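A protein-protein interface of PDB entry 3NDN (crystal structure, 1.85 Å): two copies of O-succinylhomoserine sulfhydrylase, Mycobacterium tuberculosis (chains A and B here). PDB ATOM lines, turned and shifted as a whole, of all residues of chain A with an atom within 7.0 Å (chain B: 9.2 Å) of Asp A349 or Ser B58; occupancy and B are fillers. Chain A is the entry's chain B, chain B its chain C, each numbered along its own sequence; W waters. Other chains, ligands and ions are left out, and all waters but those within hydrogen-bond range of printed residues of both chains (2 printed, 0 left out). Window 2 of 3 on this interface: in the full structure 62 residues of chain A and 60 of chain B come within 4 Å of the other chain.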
ATOM      1  N   GLN A 342       0.408  15.927  27.142  1.00  0.00           N
ATOM      2  CA  GLN A 342      -0.765  16.532  27.771  1.00  0.00           C
ATOM      3  C   GLN A 342      -0.449  17.900  28.376  1.00  0.00           C
ATOM      4  O   GLN A 342      -1.212  18.861  28.207  1.00  0.00           O
ATOM      5  CB  GLN A 342      -1.326  15.579  28.835  1.00  0.00           C
ATOM      6  CG  GLN A 342      -2.610  16.025  29.511  1.00  0.00           C
ATOM      7  CD  GLN A 342      -3.098  15.023  30.559  1.00  0.00           C
ATOM      8  OE1 GLN A 342      -2.509  14.889  31.636  1.00  0.00           O
ATOM      9  NE2 GLN A 342      -4.183  14.316  30.244  1.00  0.00           N
ATOM     10  N   ALA A 344       2.177  19.923  27.474  1.00  0.00           N
ATOM     11  CA  ALA A 344       2.462  20.842  26.367  1.00  0.00           C
ATOM     12  C   ALA A 344       1.178  21.340  25.708  1.00  0.00           C
ATOM     13  O   ALA A 344       1.032  22.529  25.445  1.00  0.00           O
ATOM     14  CB  ALA A 344       3.392  20.186  25.336  1.00  0.00           C
ATOM     15  N   PHE A 345       0.231  20.431  25.467  1.00  0.00           N
ATOM     16  CA  PHE A 345      -1.063  20.808  24.902  1.00  0.00           C
ATOM     17  C   PHE A 345      -1.790  21.812  25.801  1.00  0.00           C
ATOM     18  O   PHE A 345      -2.414  22.756  25.302  1.00  0.00           O
ATOM     19  CB  PHE A 345      -1.946  19.566  24.646  1.00  0.00           C
ATOM     20  CG  PHE A 345      -1.710  18.894  23.307  1.00  0.00           C
ATOM     21  CD1 PHE A 345      -0.468  18.953  22.672  1.00  0.00           C
ATOM     22  CD2 PHE A 345      -2.737  18.177  22.699  1.00  0.00           C
ATOM     23  CE1 PHE A 345      -0.251  18.337  21.437  1.00  0.00           C
ATOM     24  CE2 PHE A 345      -2.533  17.534  21.464  1.00  0.00           C
ATOM     25  CZ  PHE A 345      -1.291  17.618  20.828  1.00  0.00           C
ATOM     26  N   GLU A 346      -1.714  21.611  27.117  1.00  0.00           N
ATOM     27  CA  GLU A 346      -2.343  22.518  28.084  1.00  0.00           C
ATOM     28  C   GLU A 346      -1.765  23.945  27.985  1.00  0.00           C
ATOM     29  O   GLU A 346      -2.510  24.945  28.003  1.00  0.00           O
ATOM     30  CB  GLU A 346      -2.161  21.969  29.506  1.00  0.00           C
ATOM     31  CG  GLU A 346      -3.199  22.464  30.508  1.00  0.00           C
ATOM     32  CD  GLU A 346      -2.809  22.190  31.966  1.00  0.00           C
ATOM     33  OE1 GLU A 346      -1.938  21.324  32.223  1.00  0.00           O
ATOM     34  OE2 GLU A 346      -3.381  22.854  32.859  1.00  0.00           O
ATOM     35  N   VAL A 347      -0.444  24.024  27.856  1.00  0.00           N
ATOM     36  CA  VAL A 347       0.262  25.313  27.733  1.00  0.00           C
ATOM     37  C   VAL A 347      -0.169  26.099  26.467  1.00  0.00           C
ATOM     38  O   VAL A 347      -0.563  27.265  26.569  1.00  0.00           O
ATOM     39  CB  VAL A 347       1.801  25.132  27.822  1.00  0.00           C
ATOM     40  CG1 VAL A 347       2.530  26.423  27.479  1.00  0.00           C
ATOM     41  CG2 VAL A 347       2.214  24.661  29.229  1.00  0.00           C
ATOM     42  N   LEU A 348      -0.143  25.451  25.302  1.00  0.00           N
ATOM     43  CA  LEU A 348      -0.628  26.068  24.052  1.00  0.00           C
ATOM     44  C   LEU A 348      -2.062  26.571  24.150  1.00  0.00           C
ATOM     45  O   LEU A 348      -2.368  27.699  23.727  1.00  0.00           O
ATOM     46  CB  LEU A 348      -0.509  25.095  22.870  1.00  0.00           C
ATOM     47  CG  LEU A 348       0.794  25.108  22.065  1.00  0.00           C
ATOM     48  CD1 LEU A 348       2.010  24.778  22.917  1.00  0.00           C
ATOM     49  CD2 LEU A 348       0.693  24.136  20.891  1.00  0.00           C
ATOM     50  N   ASP A 349      -2.944  25.719  24.686  1.00  0.00           N
ATOM     51  CA  ASP A 349      -4.369  26.020  24.796  1.00  0.00           C
ATOM     52  C   ASP A 349      -4.708  27.173  25.760  1.00  0.00           C
ATOM     53  O   ASP A 349      -5.787  27.779  25.651  1.00  0.00           O
ATOM     54  CB  ASP A 349      -5.161  24.747  25.160  1.00  0.00           C
ATOM     55  CG  ASP A 349      -5.152  23.691  24.046  1.00  0.00           C
ATOM     56  OD1 ASP A 349      -4.709  23.984  22.909  1.00  0.00           O
ATOM     57  OD2 ASP A 349      -5.620  22.559  24.310  1.00  0.00           O
ATOM     58  N   LYS A 350      -3.786  27.489  26.675  1.00  0.00           N
ATOM     59  CA  LYS A 350      -3.957  28.583  27.642  1.00  0.00           C
ATOM     60  C   LYS A 350      -3.509  29.993  27.146  1.00  0.00           C
ATOM     61  O   LYS A 350      -3.873  31.015  27.744  1.00  0.00           O
ATOM     62  CB  LYS A 350      -3.283  28.211  28.979  1.00  0.00           C
ATOM     63  CG  LYS A 350      -3.750  29.042  30.177  1.00  0.00           C
ATOM     64  CD  LYS A 350      -3.465  28.359  31.530  1.00  0.00           C
ATOM     65  CE  LYS A 350      -4.191  29.107  32.663  1.00  0.00           C
ATOM     66  NZ  LYS A 350      -3.995  28.457  33.997  1.00  0.00           N
ATOM     67  N   MET A 351      -2.735  30.048  26.062  1.00  0.00           N
ATOM     68  CA  MET A 351      -2.355  31.329  25.416  1.00  0.00           C
ATOM     69  C   MET A 351      -3.565  32.179  25.039  1.00  0.00           C
ATOM     70  O   MET A 351      -4.554  31.655  24.517  1.00  0.00           O
ATOM     71  CB  MET A 351      -1.564  31.067  24.143  1.00  0.00           C
ATOM     72  CG  MET A 351      -0.388  30.153  24.331  1.00  0.00           C
ATOM     73  SD  MET A 351       0.996  31.093  24.974  1.00  0.00           S
ATOM     74  CE  MET A 351       2.302  30.205  24.152  1.00  0.00           C
ATOM     75  N   ARG A 352      -3.487  33.481  25.306  1.00  0.00           N
ATOM     76  CA  ARG A 352      -4.591  34.403  24.980  1.00  0.00           C
ATOM     77  C   ARG A 352      -4.201  35.454  23.953  1.00  0.00           C
ATOM     78  O   ARG A 352      -5.072  36.107  23.361  1.00  0.00           O
ATOM     79  CB  ARG A 352      -5.115  35.102  26.242  1.00  0.00           C
ATOM     80  CG  ARG A 352      -5.855  34.195  27.216  1.00  0.00           C
ATOM     81  CD  ARG A 352      -6.519  35.018  28.346  1.00  0.00           C
ATOM     82  NE  ARG A 352      -5.570  35.913  29.025  1.00  0.00           N
ATOM     83  CZ  ARG A 352      -5.884  36.751  30.015  1.00  0.00           C
ATOM     84  NH1 ARG A 352      -7.134  36.830  30.471  1.00  0.00           N
ATOM     85  NH2 ARG A 352      -4.940  37.514  30.558  1.00  0.00           N
ATOM     86  N   ILE A 356      -1.867  29.871  17.931  1.00  0.00           N
ATOM     87  CA  ILE A 356      -1.356  28.531  17.578  1.00  0.00           C
ATOM     88  C   ILE A 356      -1.252  28.402  16.039  1.00  0.00           C
ATOM     89  O   ILE A 356      -2.284  28.388  15.346  1.00  0.00           O
ATOM     90  CB  ILE A 356      -2.248  27.374  18.173  1.00  0.00           C
ATOM     91  CG1 ILE A 356      -2.454  27.556  19.683  1.00  0.00           C
ATOM     92  CG2 ILE A 356      -1.632  25.990  17.889  1.00  0.00           C
ATOM     93  CD1 ILE A 356      -3.575  26.669  20.267  1.00  0.00           C
ATOM     94  N   VAL A 367       2.940  30.079  18.131  1.00  0.00           N
ATOM     95  CA  VAL A 367       3.466  28.900  18.895  1.00  0.00           C
ATOM     96  C   VAL A 367       3.043  27.573  18.242  1.00  0.00           C
ATOM     97  O   VAL A 367       1.976  27.494  17.664  1.00  0.00           O
ATOM     98  CB  VAL A 367       3.011  28.924  20.378  1.00  0.00           C
ATOM     99  CG1 VAL A 367       1.478  28.847  20.496  1.00  0.00           C
ATOM    100  CG2 VAL A 367       3.691  27.783  21.203  1.00  0.00           C
ATOM    101  N   ALA A 412       0.300  31.165  30.835  1.00  0.00           N
ATOM    102  CA  ALA A 412       0.127  29.854  30.196  1.00  0.00           C
ATOM    103  C   ALA A 412       0.887  28.698  30.885  1.00  0.00           C
ATOM    104  O   ALA A 412       0.439  27.548  30.823  1.00  0.00           O
ATOM    105  CB  ALA A 412       0.497  29.926  28.708  1.00  0.00           C
ATOM    106  N   VAL B  55      -4.377  29.642  11.496  1.00  0.00           N
ATOM    107  CA  VAL B  55      -4.378  29.408  12.961  1.00  0.00           C
ATOM    108  C   VAL B  55      -5.358  28.282  13.381  1.00  0.00           C
ATOM    109  O   VAL B  55      -6.240  27.928  12.600  1.00  0.00           O
ATOM    110  CB  VAL B  55      -4.624  30.727  13.774  1.00  0.00           C
ATOM    111  CG1 VAL B  55      -3.518  31.770  13.481  1.00  0.00           C
ATOM    112  CG2 VAL B  55      -6.006  31.345  13.481  1.00  0.00           C
ATOM    113  N   TYR B  56      -5.173  27.710  14.580  1.00  0.00           N
ATOM    114  CA  TYR B  56      -6.039  26.628  15.116  1.00  0.00           C
ATOM    115  C   TYR B  56      -6.554  26.954  16.526  1.00  0.00           C
ATOM    116  O   TYR B  56      -5.904  27.692  17.284  1.00  0.00           O
ATOM    117  CB  TYR B  56      -5.293  25.275  15.144  1.00  0.00           C
ATOM    118  CG  TYR B  56      -4.506  25.014  13.888  1.00  0.00           C
ATOM    119  CD1 TYR B  56      -5.083  24.360  12.787  1.00  0.00           C
ATOM    120  CD2 TYR B  56      -3.187  25.458  13.780  1.00  0.00           C
ATOM    121  CE1 TYR B  56      -4.343  24.152  11.609  1.00  0.00           C
ATOM    122  CE2 TYR B  56      -2.449  25.254  12.626  1.00  0.00           C
ATOM    123  CZ  TYR B  56      -3.022  24.608  11.541  1.00  0.00           C
ATOM    124  OH  TYR B  56      -2.252  24.434  10.406  1.00  0.00           O
ATOM    125  N   GLY B  57      -7.721  26.414  16.873  1.00  0.00           N
ATOM    126  CA  GLY B  57      -8.335  26.686  18.178  1.00  0.00           C
ATOM    127  C   GLY B  57      -7.666  25.949  19.335  1.00  0.00           C
ATOM    128  O   GLY B  57      -7.771  26.370  20.501  1.00  0.00           O
ATOM    129  N   SER B  58      -6.959  24.863  19.017  1.00  0.00           N
ATOM    130  CA  SER B  58      -6.325  24.009  20.033  1.00  0.00           C
ATOM    131  C   SER B  58      -5.149  23.255  19.423  1.00  0.00           C
ATOM    132  O   SER B  58      -5.035  23.168  18.198  1.00  0.00           O
ATOM    133  CB  SER B  58      -7.336  23.019  20.650  1.00  0.00           C
ATOM    134  OG  SER B  58      -7.860  22.137  19.664  1.00  0.00           O
ATOM    135  N   ALA B  59      -4.265  22.733  20.278  1.00  0.00           N
ATOM    136  CA  ALA B  59      -3.123  21.929  19.817  1.00  0.00           C
ATOM    137  C   ALA B  59      -3.593  20.648  19.126  1.00  0.00           C
ATOM    138  O   ALA B  59      -2.965  20.181  18.176  1.00  0.00           O
ATOM    139  CB  ALA B  59      -2.175  21.613  20.990  1.00  0.00           C
ATOM    140  N   ALA B  60      -4.707  20.086  19.602  1.00  0.00           N
ATOM    141  CA  ALA B  60      -5.269  18.875  19.012  1.00  0.00           C
ATOM    142  C   ALA B  60      -5.698  19.070  17.559  1.00  0.00           C
ATOM    143  O   ALA B  60      -5.382  18.241  16.704  1.00  0.00           O
ATOM    144  CB  ALA B  60      -6.442  18.359  19.853  1.00  0.00           C
ATOM    145  N   VAL B  61      -6.456  20.136  17.300  1.00  0.00           N
ATOM    146  CA  VAL B  61      -6.895  20.486  15.943  1.00  0.00           C
ATOM    147  C   VAL B  61      -5.693  20.724  15.017  1.00  0.00           C
ATOM    148  O   VAL B  61      -5.699  20.304  13.862  1.00  0.00           O
ATOM    149  CB  VAL B  61      -7.880  21.704  15.952  1.00  0.00           C
ATOM    150  CG1 VAL B  61      -8.069  22.272  14.545  1.00  0.00           C
ATOM    151  CG2 VAL B  61      -9.239  21.296  16.547  1.00  0.00           C
ATOM    152  N   ALA B  62      -4.636  21.349  15.538  1.00  0.00           N
ATOM    153  CA  ALA B  62      -3.397  21.492  14.762  1.00  0.00           C
ATOM    154  C   ALA B  62      -2.795  20.153  14.323  1.00  0.00           C
ATOM    155  O   ALA B  62      -2.436  19.992  13.155  1.00  0.00           O
ATOM    156  CB  ALA B  62      -2.359  22.335  15.546  1.00  0.00           C
ATOM    157  N   GLU B  63      -2.693  19.200  15.255  1.00  0.00           N
ATOM    158  CA  GLU B  63      -2.163  17.854  14.973  1.00  0.00           C
ATOM    159  C   GLU B  63      -3.018  17.123  13.912  1.00  0.00           C
ATOM    160  O   GLU B  63      -2.487  16.588  12.934  1.00  0.00           O
ATOM    161  CB  GLU B  63      -2.079  17.024  16.281  1.00  0.00           C
ATOM    162  CG  GLU B  63      -1.720  15.508  16.097  1.00  0.00           C
ATOM    163  CD  GLU B  63      -1.663  14.704  17.409  1.00  0.00           C
ATOM    164  OE1 GLU B  63      -2.232  15.121  18.442  1.00  0.00           O
ATOM    165  OE2 GLU B  63      -1.041  13.618  17.405  1.00  0.00           O
ATOM    166  N   LYS B  64      -4.336  17.125  14.107  1.00  0.00           N
ATOM    167  CA  LYS B  64      -5.264  16.460  13.183  1.00  0.00           C
ATOM    168  C   LYS B  64      -5.277  17.081  11.766  1.00  0.00           C
ATOM    169  O   LYS B  64      -5.366  16.355  10.763  1.00  0.00           O
ATOM    170  CB  LYS B  64      -6.670  16.440  13.784  1.00  0.00           C
ATOM    171  CG  LYS B  64      -6.822  15.432  14.942  1.00  0.00           C
ATOM    172  CD  LYS B  64      -8.159  15.589  15.639  1.00  0.00           C
ATOM    173  CE  LYS B  64      -8.336  14.519  16.707  1.00  0.00           C
ATOM    174  NZ  LYS B  64      -9.557  14.756  17.523  1.00  0.00           N
ATOM    175  N   SER B  65      -5.168  18.407  11.695  1.00  0.00           N
ATOM    176  CA  SER B  65      -5.114  19.126  10.410  1.00  0.00           C
ATOM    177  C   SER B  65      -3.849  18.790   9.626  1.00  0.00           C
ATOM    178  O   SER B  65      -3.910  18.524   8.418  1.00  0.00           O
ATOM    179  CB  SER B  65      -5.200  20.639  10.617  1.00  0.00           C
ATOM    180  OG  SER B  65      -6.379  20.976  11.325  1.00  0.00           O
ATOM    181  N   LEU B  70      -8.597  16.254   9.262  1.00  0.00           N
ATOM    182  CA  LEU B  70      -9.581  17.336   9.071  1.00  0.00           C
ATOM    183  C   LEU B  70      -9.222  18.118   7.809  1.00  0.00           C
ATOM    184  O   LEU B  70      -8.064  18.135   7.407  1.00  0.00           O
ATOM    185  CB  LEU B  70      -9.589  18.292  10.276  1.00  0.00           C
ATOM    186  CG  LEU B  70     -10.054  17.782  11.638  1.00  0.00           C
ATOM    187  CD1 LEU B  70      -9.702  18.776  12.756  1.00  0.00           C
ATOM    188  CD2 LEU B  70     -11.568  17.482  11.628  1.00  0.00           C
ATOM    189  N   HIS B  72      -9.276  21.406   7.349  1.00  0.00           N
ATOM    190  CA  HIS B  72      -8.777  22.752   7.722  1.00  0.00           C
ATOM    191  C   HIS B  72      -7.553  23.108   6.849  1.00  0.00           C
ATOM    192  O   HIS B  72      -6.692  22.244   6.613  1.00  0.00           O
ATOM    193  CB  HIS B  72      -8.385  22.685   9.214  1.00  0.00           C
ATOM    194  CG  HIS B  72      -8.223  24.009   9.903  1.00  0.00           C
ATOM    195  ND1 HIS B  72      -7.198  24.886   9.613  1.00  0.00           N
ATOM    196  CD2 HIS B  72      -8.907  24.562  10.936  1.00  0.00           C
ATOM    197  CE1 HIS B  72      -7.281  25.938  10.411  1.00  0.00           C
ATOM    198  NE2 HIS B  72      -8.304  25.762  11.231  1.00  0.00           N
HETATM  199  O   HOH W   1      -4.712  30.123  18.121  1.00  0.00           O
HETATM  200  O   HOH W   2      -5.588  20.411  22.481  1.00  0.00           O
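The backbone NH (N) of Tyr B56 lies within hydrogen-bond range of the backbone carbonyl oxygen (O) of Ile A356, 3.1 Å away.
OD1 of Asp A349 lies within hydrogen-bond range of N of Ala B59 (2.9 Å).
The side-chain hydroxyl of Ser B58 sits at hydrogen-bond distance from the backbone NH of Val B61 (3.4 Å).
NE2 of His B72 lies close to O of Val B55, 3.3 Å away.
Among the printed residues, merely in contact across the chains: Asp A349 with Ser B58, Ile A356 with Val B55, Phe A345 with Glu B63, Phe A345 with Ala B59, Leu A348 with Ala B59, Ile A356 with Ser B58, Phe A345 with Ala B60 and Ile A356 with Ala B59.
Asp A349 touches two residues of chain B.
Ser B58 touches just these residues of chain A: Asp A349 (3.3 Å) and Ile A356 (3.8 Å).
Printed residues of chain A within 4 Å of Ala B60: Phe A345 (3.8 Å).
Of the printed residues of chain B, Leu A348 touches Ala B59.
Printed residues of chain B within 4 Å of Ile A356: Val B55, Tyr B56, Ser B58 and Ala B59.
Arg A352 touches none of the printed residues of chain B.
The nearest residue of chain B that does not touch Asp A349 is Gly B57 (4.6 Å).
Of the 13 printed residues of chain A, 4 touch a printed residue of chain B.
Among the printed residues, 10 pairs touch across the chains.
No position is printed for both chains.
Water W2 lies within hydrogen-bond range of OD2 of Asp A349, N of Ala B60 and N of Ala B59.
Water W1 lies within hydrogen-bond range of O of Tyr B56 (2.8 Å) and N of Ile A356 (2.9 Å).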
